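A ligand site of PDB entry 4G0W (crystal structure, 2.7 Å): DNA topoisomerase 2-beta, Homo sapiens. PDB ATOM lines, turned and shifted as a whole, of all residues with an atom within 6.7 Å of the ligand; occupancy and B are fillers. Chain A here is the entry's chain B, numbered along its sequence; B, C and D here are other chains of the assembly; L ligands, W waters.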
ATOM      1  N   LEU A  84     -13.189 -21.501  29.598  1.00  0.00           N
ATOM      2  CA  LEU A  84     -12.540 -20.229  29.344  1.00  0.00           C
ATOM      3  C   LEU A  84     -13.612 -19.155  29.228  1.00  0.00           C
ATOM      4  O   LEU A  84     -14.551 -19.285  28.440  1.00  0.00           O
ATOM      5  CB  LEU A  84     -11.764 -20.270  28.023  1.00  0.00           C
ATOM      6  CG  LEU A  84     -10.804 -21.411  27.728  1.00  0.00           C
ATOM      7  CD1 LEU A  84     -10.128 -21.176  26.370  1.00  0.00           C
ATOM      8  CD2 LEU A  84      -9.777 -21.565  28.845  1.00  0.00           C
ATOM      9  N   ARG A  85     -13.470 -18.076  29.988  1.00  0.00           N
ATOM     10  CA  ARG A  85     -14.369 -16.944  29.828  1.00  0.00           C
ATOM     11  C   ARG A  85     -13.742 -15.848  28.966  1.00  0.00           C
ATOM     12  O   ARG A  85     -12.761 -15.217  29.355  1.00  0.00           O
ATOM     13  CB  ARG A  85     -14.755 -16.368  31.193  1.00  0.00           C
ATOM     14  CG  ARG A  85     -15.939 -17.084  31.831  1.00  0.00           C
ATOM     15  CD  ARG A  85     -16.575 -16.207  32.893  1.00  0.00           C
ATOM     16  NE  ARG A  85     -15.963 -16.389  34.197  1.00  0.00           N
ATOM     17  CZ  ARG A  85     -15.800 -15.418  35.079  1.00  0.00           C
ATOM     18  NH1 ARG A  85     -16.189 -14.187  34.769  1.00  0.00           N
ATOM     19  NH2 ARG A  85     -15.243 -15.664  36.260  1.00  0.00           N
ATOM     20  N   GLY A  86     -14.327 -15.621  27.797  1.00  0.00           N
ATOM     21  CA  GLY A  86     -13.866 -14.528  26.956  1.00  0.00           C
ATOM     22  C   GLY A  86     -12.849 -14.887  25.889  1.00  0.00           C
ATOM     23  O   GLY A  86     -12.366 -16.013  25.813  1.00  0.00           O
ATOM     24  N   LYS A  87     -12.549 -13.922  25.034  1.00  0.00           N
ATOM     25  CA  LYS A  87     -11.507 -14.076  24.047  1.00  0.00           C
ATOM     26  C   LYS A  87     -10.167 -14.232  24.783  1.00  0.00           C
ATOM     27  O   LYS A  87      -9.984 -13.695  25.886  1.00  0.00           O
ATOM     28  CB  LYS A  87     -11.469 -12.884  23.107  1.00  0.00           C
ATOM     29  CG  LYS A  87     -12.727 -12.712  22.260  1.00  0.00           C
ATOM     30  CD  LYS A  87     -12.970 -13.926  21.395  1.00  0.00           C
ATOM     31  CE  LYS A  87     -14.239 -13.813  20.584  1.00  0.00           C
ATOM     32  NZ  LYS A  87     -14.031 -13.066  19.327  1.00  0.00           N
ATOM     33  N   ILE A  88      -9.249 -14.979  24.193  1.00  0.00           N
ATOM     34  CA  ILE A  88      -8.000 -15.235  24.879  1.00  0.00           C
ATOM     35  C   ILE A  88      -6.839 -14.559  24.168  1.00  0.00           C
ATOM     36  O   ILE A  88      -6.958 -14.136  23.024  1.00  0.00           O
ATOM     37  CB  ILE A  88      -7.728 -16.739  25.020  1.00  0.00           C
ATOM     38  CG1 ILE A  88      -7.291 -17.353  23.695  1.00  0.00           C
ATOM     39  CG2 ILE A  88      -8.959 -17.446  25.567  1.00  0.00           C
ATOM     40  CD1 ILE A  88      -6.616 -18.691  23.892  1.00  0.00           C
ATOM     41  N   LEU A  89      -5.714 -14.457  24.875  1.00  0.00           N
ATOM     42  CA  LEU A  89      -4.520 -13.795  24.361  1.00  0.00           C
ATOM     43  C   LEU A  89      -4.022 -14.398  23.038  1.00  0.00           C
ATOM     44  O   LEU A  89      -3.901 -15.615  22.917  1.00  0.00           O
ATOM     45  CB  LEU A  89      -3.422 -13.863  25.425  1.00  0.00           C
ATOM     46  CG  LEU A  89      -2.081 -13.206  25.174  1.00  0.00           C
ATOM     47  CD1 LEU A  89      -2.221 -11.718  24.979  1.00  0.00           C
ATOM     48  CD2 LEU A  89      -1.185 -13.490  26.344  1.00  0.00           C
ATOM     49  N   ASN A 102      -0.809 -13.883  32.105  1.00  0.00           N
ATOM     50  CA  ASN A 102      -2.142 -14.230  31.623  1.00  0.00           C
ATOM     51  C   ASN A 102      -2.703 -15.499  32.268  1.00  0.00           C
ATOM     52  O   ASN A 102      -2.056 -16.558  32.245  1.00  0.00           O
ATOM     53  CB  ASN A 102      -2.121 -14.381  30.110  1.00  0.00           C
ATOM     54  CG  ASN A 102      -3.477 -14.670  29.540  1.00  0.00           C
ATOM     55  OD1 ASN A 102      -3.845 -15.830  29.311  1.00  0.00           O
ATOM     56  ND2 ASN A 102      -4.254 -13.606  29.289  1.00  0.00           N
ATOM     57  N   ALA A 103      -3.905 -15.410  32.826  1.00  0.00           N
ATOM     58  CA  ALA A 103      -4.493 -16.526  33.580  1.00  0.00           C
ATOM     59  C   ALA A 103      -4.871 -17.759  32.747  1.00  0.00           C
ATOM     60  O   ALA A 103      -4.572 -18.867  33.159  1.00  0.00           O
ATOM     61  CB  ALA A 103      -5.690 -16.055  34.394  1.00  0.00           C
ATOM     62  N   GLU A 104      -5.538 -17.581  31.615  1.00  0.00           N
ATOM     63  CA  GLU A 104      -5.963 -18.754  30.858  1.00  0.00           C
ATOM     64  C   GLU A 104      -4.803 -19.593  30.326  1.00  0.00           C
ATOM     65  O   GLU A 104      -4.787 -20.813  30.522  1.00  0.00           O
ATOM     66  CB  GLU A 104      -6.921 -18.417  29.723  1.00  0.00           C
ATOM     67  CG  GLU A 104      -8.364 -18.228  30.150  1.00  0.00           C
ATOM     68  CD  GLU A 104      -8.625 -16.844  30.720  1.00  0.00           C
ATOM     69  OE1 GLU A 104      -7.700 -15.996  30.698  1.00  0.00           O
ATOM     70  OE2 GLU A 104      -9.767 -16.607  31.191  1.00  0.00           O
ATOM     71  N   ILE A 105      -3.844 -18.971  29.653  1.00  0.00           N
ATOM     72  CA  ILE A 105      -2.694 -19.682  29.073  1.00  0.00           C
ATOM     73  C   ILE A 105      -1.913 -20.440  30.127  1.00  0.00           C
ATOM     74  O   ILE A 105      -1.540 -21.603  29.973  1.00  0.00           O
ATOM     75  CB  ILE A 105      -1.768 -18.711  28.321  1.00  0.00           C
ATOM     76  CG1 ILE A 105      -2.343 -18.402  26.949  1.00  0.00           C
ATOM     77  CG2 ILE A 105      -0.372 -19.294  28.160  1.00  0.00           C
ATOM     78  CD1 ILE A 105      -2.328 -16.940  26.643  1.00  0.00           C
ATOM     79  N   GLY A 358     -24.534 -10.578  23.749  1.00  0.00           N
ATOM     80  CA  GLY A 358     -24.706 -10.204  25.128  1.00  0.00           C
ATOM     81  C   GLY A 358     -25.171  -8.768  25.202  1.00  0.00           C
ATOM     82  O   GLY A 358     -24.808  -7.943  24.368  1.00  0.00           O
ATOM     83  N   GLN A 360     -24.623  -6.501  27.571  1.00  0.00           N
ATOM     84  CA  GLN A 360     -23.683  -5.526  28.107  1.00  0.00           C
ATOM     85  C   GLN A 360     -23.022  -4.717  26.997  1.00  0.00           C
ATOM     86  O   GLN A 360     -22.833  -3.483  27.119  1.00  0.00           O
ATOM     87  CB  GLN A 360     -22.623  -6.204  28.968  1.00  0.00           C
ATOM     88  CG  GLN A 360     -21.957  -5.252  29.962  1.00  0.00           C
ATOM     89  CD  GLN A 360     -20.641  -5.793  30.504  1.00  0.00           C
ATOM     90  OE1 GLN A 360     -19.675  -6.005  29.746  1.00  0.00           O
ATOM     91  NE2 GLN A 360     -20.592  -6.031  31.822  1.00  0.00           N
ATOM     92  N   ALA A 361     -22.690  -5.392  25.894  1.00  0.00           N
ATOM     93  CA  ALA A 361     -22.080  -4.715  24.759  1.00  0.00           C
ATOM     94  C   ALA A 361     -23.047  -3.673  24.215  1.00  0.00           C
ATOM     95  O   ALA A 361     -22.636  -2.583  23.829  1.00  0.00           O
ATOM     96  CB  ALA A 361     -21.712  -5.706  23.684  1.00  0.00           C
ATOM     97  N   MET A 364     -23.261  -0.625  26.460  1.00  0.00           N
ATOM     98  CA  MET A 364     -22.107   0.229  26.239  1.00  0.00           C
ATOM     99  C   MET A 364     -22.238   1.037  24.939  1.00  0.00           C
ATOM    100  O   MET A 364     -21.890   2.215  24.900  1.00  0.00           O
ATOM    101  CB  MET A 364     -20.824  -0.604  26.265  1.00  0.00           C
ATOM    102  CG  MET A 364     -20.469  -1.115  27.660  1.00  0.00           C
ATOM    103  SD  MET A 364     -19.073  -2.284  27.630  1.00  0.00           S
ATOM    104  CE  MET A 364     -17.687  -1.182  27.369  1.00  0.00           C
ATOM    105  P    DC B   3     -15.351  -1.048  40.417  1.00  0.00           P
ATOM    106  OP1  DC B   3     -14.254  -0.251  40.987  1.00  0.00           O
ATOM    107  OP2  DC B   3     -15.962  -0.670  39.119  1.00  0.00           O
ATOM    108  O5'  DC B   3     -14.802  -2.548  40.341  1.00  0.00           O
ATOM    109  C5'  DC B   3     -14.072  -3.064  41.451  1.00  0.00           C
ATOM    110  C4'  DC B   3     -13.701  -4.522  41.231  1.00  0.00           C
ATOM    111  O4'  DC B   3     -14.881  -5.347  41.229  1.00  0.00           O
ATOM    112  C3'  DC B   3     -13.057  -4.808  39.885  1.00  0.00           C
ATOM    113  O3'  DC B   3     -11.667  -4.604  39.955  1.00  0.00           O
ATOM    114  C2'  DC B   3     -13.372  -6.282  39.637  1.00  0.00           C
ATOM    115  C1'  DC B   3     -14.712  -6.435  40.325  1.00  0.00           C
ATOM    116  N1   DC B   3     -15.865  -6.445  39.395  1.00  0.00           N
ATOM    117  C2   DC B   3     -16.252  -7.660  38.823  1.00  0.00           C
ATOM    118  O2   DC B   3     -15.584  -8.671  39.090  1.00  0.00           O
ATOM    119  N3   DC B   3     -17.321  -7.675  37.986  1.00  0.00           N
ATOM    120  C4   DC B   3     -17.975  -6.536  37.743  1.00  0.00           C
ATOM    121  N4   DC B   3     -19.019  -6.559  36.924  1.00  0.00           N
ATOM    122  C5   DC B   3     -17.588  -5.305  38.333  1.00  0.00           C
ATOM    123  C6   DC B   3     -16.536  -5.292  39.144  1.00  0.00           C
ATOM    124  P    DA B   4     -10.858  -4.188  38.623  1.00  0.00           P
ATOM    125  OP1  DA B   4      -9.527  -3.681  39.050  1.00  0.00           O
ATOM    126  OP2  DA B   4     -11.752  -3.336  37.801  1.00  0.00           O
ATOM    127  O5'  DA B   4     -10.665  -5.585  37.856  1.00  0.00           O
ATOM    128  C5'  DA B   4     -10.075  -6.710  38.495  1.00  0.00           C
ATOM    129  C4'  DA B   4     -10.180  -7.934  37.586  1.00  0.00           C
ATOM    130  O4'  DA B   4     -11.506  -8.496  37.660  1.00  0.00           O
ATOM    131  C3'  DA B   4      -9.938  -7.668  36.112  1.00  0.00           C
ATOM    132  O3'  DA B   4      -8.554  -7.849  35.851  1.00  0.00           O
ATOM    133  C2'  DA B   4     -10.761  -8.748  35.425  1.00  0.00           C
ATOM    134  C1'  DA B   4     -11.882  -9.039  36.407  1.00  0.00           C
ATOM    135  N9   DA B   4     -13.150  -8.465  35.995  1.00  0.00           N
ATOM    136  C8   DA B   4     -13.547  -7.164  36.152  1.00  0.00           C
ATOM    137  N7   DA B   4     -14.749  -6.915  35.668  1.00  0.00           N
ATOM    138  C5   DA B   4     -15.158  -8.136  35.172  1.00  0.00           C
ATOM    139  C6   DA B   4     -16.351  -8.533  34.519  1.00  0.00           C
ATOM    140  N6   DA B   4     -17.369  -7.716  34.277  1.00  0.00           N
ATOM    141  N1   DA B   4     -16.447  -9.814  34.119  1.00  0.00           N
ATOM    142  C2   DA B   4     -15.420 -10.646  34.374  1.00  0.00           C
ATOM    143  N3   DA B   4     -14.257 -10.377  34.977  1.00  0.00           N
ATOM    144  C4   DA B   4     -14.196  -9.098  35.361  1.00  0.00           C
ATOM    145  P    DG B   5      -7.827  -7.023  34.680  1.00  0.00           P
ATOM    146  OP1  DG B   5      -6.368  -7.050  34.960  1.00  0.00           O
ATOM    147  OP2  DG B   5      -8.521  -5.720  34.508  1.00  0.00           O
ATOM    148  O5'  DG B   5      -8.128  -7.876  33.369  1.00  0.00           O
ATOM    149  C5'  DG B   5      -7.725  -9.235  33.275  1.00  0.00           C
ATOM    150  C4'  DG B   5      -7.656  -9.656  31.811  1.00  0.00           C
ATOM    151  O4'  DG B   5      -8.975  -9.518  31.216  1.00  0.00           O
ATOM    152  C3'  DG B   5      -6.694  -8.870  30.907  1.00  0.00           C
ATOM    153  O3'  DG B   5      -6.278  -9.747  29.890  1.00  0.00           O
ATOM    154  C2'  DG B   5      -7.636  -7.844  30.290  1.00  0.00           C
ATOM    155  C1'  DG B   5      -8.837  -8.758  30.034  1.00  0.00           C
ATOM    156  N9   DG B   5     -10.127  -8.131  29.754  1.00  0.00           N
ATOM    157  C8   DG B   5     -10.597  -6.939  30.219  1.00  0.00           C
ATOM    158  N7   DG B   5     -11.799  -6.667  29.807  1.00  0.00           N
ATOM    159  C5   DG B   5     -12.157  -7.750  29.026  1.00  0.00           C
ATOM    160  C6   DG B   5     -13.354  -8.012  28.335  1.00  0.00           C
ATOM    161  O6   DG B   5     -14.366  -7.285  28.283  1.00  0.00           O
ATOM    162  N1   DG B   5     -13.329  -9.241  27.663  1.00  0.00           N
ATOM    163  C2   DG B   5     -12.255 -10.103  27.678  1.00  0.00           C
ATOM    164  N2   DG B   5     -12.393 -11.234  26.960  1.00  0.00           N
ATOM    165  N3   DG B   5     -11.124  -9.865  28.341  1.00  0.00           N
ATOM    166  C4   DG B   5     -11.138  -8.674  28.993  1.00  0.00           C
ATOM    167  P    DC B   6      -4.723  -9.922  29.507  1.00  0.00           P
ATOM    168  OP1  DC B   6      -4.144 -10.925  30.408  1.00  0.00           O
ATOM    169  OP2  DC B   6      -4.089  -8.574  29.452  1.00  0.00           O
ATOM    170  O5'  DC B   6      -4.798 -10.503  28.018  1.00  0.00           O
ATOM    171  C5'  DC B   6      -5.248  -9.659  26.927  1.00  0.00           C
ATOM    172  C4'  DC B   6      -6.313 -10.338  26.078  1.00  0.00           C
ATOM    173  O4'  DC B   6      -7.603 -10.165  26.686  1.00  0.00           O
ATOM    174  C3'  DC B   6      -6.481  -9.780  24.677  1.00  0.00           C
ATOM    175  O3'  DC B   6      -5.655 -10.507  23.855  1.00  0.00           O
ATOM    176  C2'  DC B   6      -7.888 -10.215  24.338  1.00  0.00           C
ATOM    177  C1'  DC B   6      -8.589 -10.108  25.683  1.00  0.00           C
ATOM    178  N1   DC B   6      -9.409  -8.878  25.830  1.00  0.00           N
ATOM    179  C2   DC B   6     -10.632  -8.823  25.180  1.00  0.00           C
ATOM    180  O2   DC B   6     -10.976  -9.802  24.514  1.00  0.00           O
ATOM    181  N3   DC B   6     -11.409  -7.706  25.298  1.00  0.00           N
ATOM    182  C4   DC B   6     -10.982  -6.685  26.036  1.00  0.00           C
ATOM    183  N4   DC B   6     -11.781  -5.623  26.136  1.00  0.00           N
ATOM    184  C5   DC B   6      -9.728  -6.716  26.699  1.00  0.00           C
ATOM    185  C6   DC B   6      -8.976  -7.819  26.579  1.00  0.00           C
ATOM    186  P    DT C   1     -23.965 -12.754  28.495  1.00  0.00           P
ATOM    187  OP1  DT C   1     -24.678 -11.751  29.315  1.00  0.00           O
ATOM    188  OP2  DT C   1     -23.068 -12.345  27.390  1.00  0.00           O
ATOM    189  O5'  DT C   1     -23.093 -13.692  29.463  1.00  0.00           O
ATOM    190  C5'  DT C   1     -22.406 -14.806  28.933  1.00  0.00           C
ATOM    191  C4'  DT C   1     -21.230 -15.157  29.796  1.00  0.00           C
ATOM    192  O4'  DT C   1     -20.207 -14.148  29.616  1.00  0.00           O
ATOM    193  C3'  DT C   1     -21.506 -15.195  31.297  1.00  0.00           C
ATOM    194  O3'  DT C   1     -22.043 -16.475  31.723  1.00  0.00           O
ATOM    195  C2'  DT C   1     -20.095 -14.949  31.842  1.00  0.00           C
ATOM    196  C1'  DT C   1     -19.491 -14.000  30.831  1.00  0.00           C
ATOM    197  N1   DT C   1     -19.574 -12.617  31.346  1.00  0.00           N
ATOM    198  C2   DT C   1     -18.578 -12.219  32.191  1.00  0.00           C
ATOM    199  O2   DT C   1     -17.644 -12.948  32.507  1.00  0.00           O
ATOM    200  N3   DT C   1     -18.713 -10.931  32.658  1.00  0.00           N
ATOM    201  C4   DT C   1     -19.712 -10.039  32.355  1.00  0.00           C
ATOM    202  O4   DT C   1     -19.729  -8.918  32.835  1.00  0.00           O
ATOM    203  C5   DT C   1     -20.733 -10.528  31.470  1.00  0.00           C
ATOM    204  C7   DT C   1     -21.875  -9.633  31.075  1.00  0.00           C
ATOM    205  C6   DT C   1     -20.620 -11.782  31.005  1.00  0.00           C
ATOM    206  P    DG C   2     -22.807 -16.609  33.150  1.00  0.00           P
ATOM    207  OP1  DG C   2     -23.528 -17.898  33.145  1.00  0.00           O
ATOM    208  OP2  DG C   2     -23.524 -15.331  33.420  1.00  0.00           O
ATOM    209  O5'  DG C   2     -21.609 -16.683  34.220  1.00  0.00           O
ATOM    210  C5'  DG C   2     -20.513 -17.557  34.067  1.00  0.00           C
ATOM    211  C4'  DG C   2     -19.440 -17.138  35.031  1.00  0.00           C
ATOM    212  O4'  DG C   2     -19.081 -15.772  34.739  1.00  0.00           O
ATOM    213  C3'  DG C   2     -19.886 -17.182  36.492  1.00  0.00           C
ATOM    214  O3'  DG C   2     -18.912 -17.800  37.331  1.00  0.00           O
ATOM    215  C2'  DG C   2     -20.027 -15.713  36.863  1.00  0.00           C
ATOM    216  C1'  DG C   2     -19.055 -15.017  35.935  1.00  0.00           C
ATOM    217  N9   DG C   2     -19.550 -13.653  35.778  1.00  0.00           N
ATOM    218  C8   DG C   2     -20.753 -13.260  35.222  1.00  0.00           C
ATOM    219  N7   DG C   2     -20.929 -11.976  35.277  1.00  0.00           N
ATOM    220  C5   DG C   2     -19.798 -11.486  35.929  1.00  0.00           C
ATOM    221  C6   DG C   2     -19.446 -10.169  36.285  1.00  0.00           C
ATOM    222  O6   DG C   2     -20.085  -9.122  36.063  1.00  0.00           O
ATOM    223  N1   DG C   2     -18.223 -10.110  36.938  1.00  0.00           N
ATOM    224  C2   DG C   2     -17.428 -11.205  37.215  1.00  0.00           C
ATOM    225  N2   DG C   2     -16.263 -10.942  37.840  1.00  0.00           N
ATOM    226  N3   DG C   2     -17.733 -12.450  36.879  1.00  0.00           N
ATOM    227  C4   DG C   2     -18.937 -12.515  36.237  1.00  0.00           C
ATOM    228  P    DA D   6     -19.197   0.452  19.436  1.00  0.00           P
ATOM    229  OP1  DA D   6     -19.082   1.327  18.259  1.00  0.00           O
ATOM    230  OP2  DA D   6     -20.081   0.823  20.582  1.00  0.00           O
ATOM    231  O5'  DA D   6     -19.665  -0.998  18.972  1.00  0.00           O
ATOM    232  C5'  DA D   6     -19.279  -1.564  17.734  1.00  0.00           C
ATOM    233  C4'  DA D   6     -19.119  -3.065  17.887  1.00  0.00           C
ATOM    234  O4'  DA D   6     -17.876  -3.311  18.581  1.00  0.00           O
ATOM    235  C3'  DA D   6     -20.213  -3.787  18.700  1.00  0.00           C
ATOM    236  O3'  DA D   6     -20.415  -5.063  18.136  1.00  0.00           O
ATOM    237  C2'  DA D   6     -19.561  -3.897  20.067  1.00  0.00           C
ATOM    238  C1'  DA D   6     -18.128  -4.193  19.658  1.00  0.00           C
ATOM    239  N9   DA D   6     -17.105  -3.945  20.670  1.00  0.00           N
ATOM    240  C8   DA D   6     -17.116  -3.009  21.667  1.00  0.00           C
ATOM    241  N7   DA D   6     -16.037  -2.993  22.410  1.00  0.00           N
ATOM    242  C5   DA D   6     -15.258  -4.000  21.857  1.00  0.00           C
ATOM    243  C6   DA D   6     -13.993  -4.487  22.177  1.00  0.00           C
ATOM    244  N6   DA D   6     -13.262  -4.018  23.184  1.00  0.00           N
ATOM    245  N1   DA D   6     -13.497  -5.486  21.427  1.00  0.00           N
ATOM    246  C2   DA D   6     -14.224  -5.952  20.406  1.00  0.00           C
ATOM    247  N3   DA D   6     -15.427  -5.566  19.997  1.00  0.00           N
ATOM    248  C4   DA D   6     -15.895  -4.588  20.772  1.00  0.00           C
ATOM    249  P    DG D   7     -21.836  -5.800  18.298  1.00  0.00           P
ATOM    250  OP1  DG D   7     -22.489  -5.838  16.980  1.00  0.00           O
ATOM    251  OP2  DG D   7     -22.508  -5.250  19.480  1.00  0.00           O
ATOM    252  O5'  DG D   7     -21.434  -7.327  18.620  1.00  0.00           O
ATOM    253  C5'  DG D   7     -20.982  -7.743  19.910  1.00  0.00           C
ATOM    254  C4'  DG D   7     -19.798  -8.708  19.816  1.00  0.00           C
ATOM    255  O4'  DG D   7     -18.558  -7.953  19.854  1.00  0.00           O
ATOM    256  C3'  DG D   7     -19.711  -9.692  20.971  1.00  0.00           C
ATOM    257  O3'  DG D   7     -20.452 -10.873  20.681  1.00  0.00           O
ATOM    258  C2'  DG D   7     -18.229  -9.992  21.004  1.00  0.00           C
ATOM    259  C1'  DG D   7     -17.603  -8.655  20.626  1.00  0.00           C
ATOM    260  N9   DG D   7     -17.194  -7.860  21.771  1.00  0.00           N
ATOM    261  C8   DG D   7     -17.892  -6.886  22.447  1.00  0.00           C
ATOM    262  N7   DG D   7     -17.210  -6.342  23.437  1.00  0.00           N
ATOM    263  C5   DG D   7     -15.990  -7.009  23.424  1.00  0.00           C
ATOM    264  C6   DG D   7     -14.851  -6.876  24.245  1.00  0.00           C
ATOM    265  O6   DG D   7     -14.662  -6.114  25.198  1.00  0.00           O
ATOM    266  N1   DG D   7     -13.842  -7.757  23.884  1.00  0.00           N
ATOM    267  C2   DG D   7     -13.917  -8.650  22.847  1.00  0.00           C
ATOM    268  N2   DG D   7     -12.836  -9.409  22.619  1.00  0.00           N
ATOM    269  N3   DG D   7     -14.968  -8.793  22.052  1.00  0.00           N
ATOM    270  C4   DG D   7     -15.967  -7.943  22.408  1.00  0.00           C
ATOM    271  P    DC D   8     -21.031 -11.795  21.859  1.00  0.00           P
ATOM    272  OP1  DC D   8     -21.943 -12.768  21.256  1.00  0.00           O
ATOM    273  OP2  DC D   8     -21.491 -10.905  22.972  1.00  0.00           O
ATOM    274  O5'  DC D   8     -19.738 -12.556  22.414  1.00  0.00           O
ATOM    275  C5'  DC D   8     -18.960 -13.435  21.607  1.00  0.00           C
ATOM    276  C4'  DC D   8     -17.784 -13.934  22.431  1.00  0.00           C
ATOM    277  O4'  DC D   8     -16.949 -12.804  22.791  1.00  0.00           O
ATOM    278  C3'  DC D   8     -18.155 -14.647  23.732  1.00  0.00           C
ATOM    279  O3'  DC D   8     -17.354 -15.819  23.942  1.00  0.00           O
ATOM    280  C2'  DC D   8     -17.855 -13.619  24.807  1.00  0.00           C
ATOM    281  C1'  DC D   8     -16.718 -12.819  24.192  1.00  0.00           C
ATOM    282  N1   DC D   8     -16.717 -11.451  24.797  1.00  0.00           N
ATOM    283  C2   DC D   8     -15.581 -11.004  25.492  1.00  0.00           C
ATOM    284  O2   DC D   8     -14.601 -11.747  25.549  1.00  0.00           O
ATOM    285  N3   DC D   8     -15.593  -9.795  26.074  1.00  0.00           N
ATOM    286  C4   DC D   8     -16.681  -9.030  25.997  1.00  0.00           C
ATOM    287  N4   DC D   8     -16.655  -7.832  26.600  1.00  0.00           N
ATOM    288  C5   DC D   8     -17.845  -9.472  25.297  1.00  0.00           C
ATOM    289  C6   DC D   8     -17.827 -10.674  24.725  1.00  0.00           C
HETATM  290  O1  LIG L   1     -14.745 -12.657  29.873  1.00  0.00           O
HETATM  291  C1  LIG L   1     -15.223 -11.541  30.067  1.00  0.00           C
HETATM  292  C2  LIG L   1     -16.499 -11.205  29.489  1.00  0.00           C
HETATM  293  C3  LIG L   1     -17.220 -12.217  28.684  1.00  0.00           C
HETATM  294  C4  LIG L   1     -18.448 -11.924  28.122  1.00  0.00           C
HETATM  295  C5  LIG L   1     -19.004 -10.633  28.329  1.00  0.00           C
HETATM  296  C6  LIG L   1     -18.297  -9.644  29.110  1.00  0.00           C
HETATM  297  C7  LIG L   1     -17.039  -9.948  29.699  1.00  0.00           C
HETATM  298  C8  LIG L   1     -16.305  -8.938  30.506  1.00  0.00           C
HETATM  299  O2  LIG L   1     -16.763  -7.828  30.711  1.00  0.00           O
HETATM  300  C9  LIG L   1     -15.044  -9.266  31.060  1.00  0.00           C
HETATM  301  C10 LIG L   1     -14.320  -8.267  31.834  1.00  0.00           C
HETATM  302  N1  LIG L   1     -14.912  -6.939  32.040  1.00  0.00           N
HETATM  303  C11 LIG L   1     -14.128  -5.780  32.394  1.00  0.00           C
HETATM  304  C12 LIG L   1     -14.608  -4.496  31.764  1.00  0.00           C
HETATM  305  N2  LIG L   1     -14.114  -4.182  30.403  1.00  0.00           N
HETATM  306  C13 LIG L   1     -15.231  -3.780  29.557  1.00  0.00           C
HETATM  307  C14 LIG L   1     -16.008  -4.823  28.903  1.00  0.00           C
HETATM  308  O3  LIG L   1     -17.217  -5.222  29.456  1.00  0.00           O
HETATM  309  C15 LIG L   1     -13.103  -8.581  32.358  1.00  0.00           C
HETATM  310  C16 LIG L   1     -12.530  -9.928  32.158  1.00  0.00           C
HETATM  311  C17 LIG L   1     -13.219 -10.875  31.405  1.00  0.00           C
HETATM  312  N3  LIG L   1     -12.665 -12.249  31.157  1.00  0.00           N
HETATM  313  C18 LIG L   1     -11.371 -12.634  31.669  1.00  0.00           C
HETATM  314  C19 LIG L   1     -10.544 -13.555  30.753  1.00  0.00           C
HETATM  315  N4  LIG L   1      -9.911 -12.938  29.595  1.00  0.00           N
HETATM  316  C20 LIG L   1      -8.498 -13.135  29.708  1.00  0.00           C
HETATM  317  C21 LIG L   1      -7.706 -13.199  28.430  1.00  0.00           C
HETATM  318  O4  LIG L   1      -6.726 -14.163  28.371  1.00  0.00           O
HETATM  319  C22 LIG L   1     -14.501 -10.545  30.853  1.00  0.00           C
HETATM  320  O   HOH W   1     -11.620  -3.704  30.967  1.00  0.00           O
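OE1 of Gln 360 is in hydrogen-bond range of O3 of the ligand (2.6 Å).
The side-chain amide nitrogen (ND2) of Asn 102 sits at hydrogen-bond distance from an oxygen (O4) of the ligand.
A nitrogen (N2) of the ligand sits close to N7 of DG 5 of chain B, at 3.4 Å.
O of Arg 85 sits close to N3 of the ligand, 3.5 Å away.
A nitrogen (N4) of the ligand lies within salt-bridge range of the side-chain carboxylate (OE1) of Glu 104 (3.9 Å).
N1 of the ligand sits close to N6 of DA 4 of chain B (3.4 Å).
NE2 of Gln 360 sits at hydrogen-bond distance from O4 of DT 1 of chain C, 3.2 Å away.
OP1 of DC 6 of chain B sits at hydrogen-bond distance from the side-chain amide nitrogen (ND2) of Asn 102 (2.9 Å).
OD1 of Asn 102 is in hydrogen-bond range of N of Ile 105, at 3.2 Å.
N2 of DG 5 of chain B is in hydrogen-bond range of N of Lys 87 (3.3 Å).
NH1 of Arg 85 sits at hydrogen-bond distance from N3 of DG 2 of chain C, 3.1 Å away.
The backbone NH of Lys 87 lies within hydrogen-bond range of O2 of DC 8 of chain D (3.0 Å).
OP2 of DC 8 of chain D lies within hydrogen-bond range of N of Gly 358 (3.2 Å).
N2 of DG 7 of chain D sits close to O2 of DC 6 of chain B (2.7 Å).
Gly 86 touches the ligand.
Lys 87 touches the ligand (O to C21, 3.5 Å).
Ile 88 touches the ligand.
N of Leu 89 touches O4 of the ligand (3.7 Å).
SD of Met 364 touches O3 of the ligand, at 3.9 Å.
O4' of DC 6 of chain B touches C21 of the ligand, at 3.5 Å.
DT 1 of chain C touches the ligand.
C5 of DC 8 of chain D touches C5 of the ligand, at 3.4 Å.
Within 4 Å of the ligand: Arg 85, Gly 86, Lys 87, Ile 88, Leu 89, Asn 102, Glu 104, Gln 360, Met 364, DA 4 of chain B, DG 5 of chain B, DC 6 of chain B, DT 1 of chain C and DC 8 of chain D.
Along chain A the residues within 4 Å of the ligand span positions 85 to 364.
The nearest printed residue that does not touch the ligand is DG 7 of chain D (4.1 Å).
Water W1 lies within hydrogen-bond range of N2 of the ligand (2.6 Å) and N7 of DG 5 of chain B (3.2 Å).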
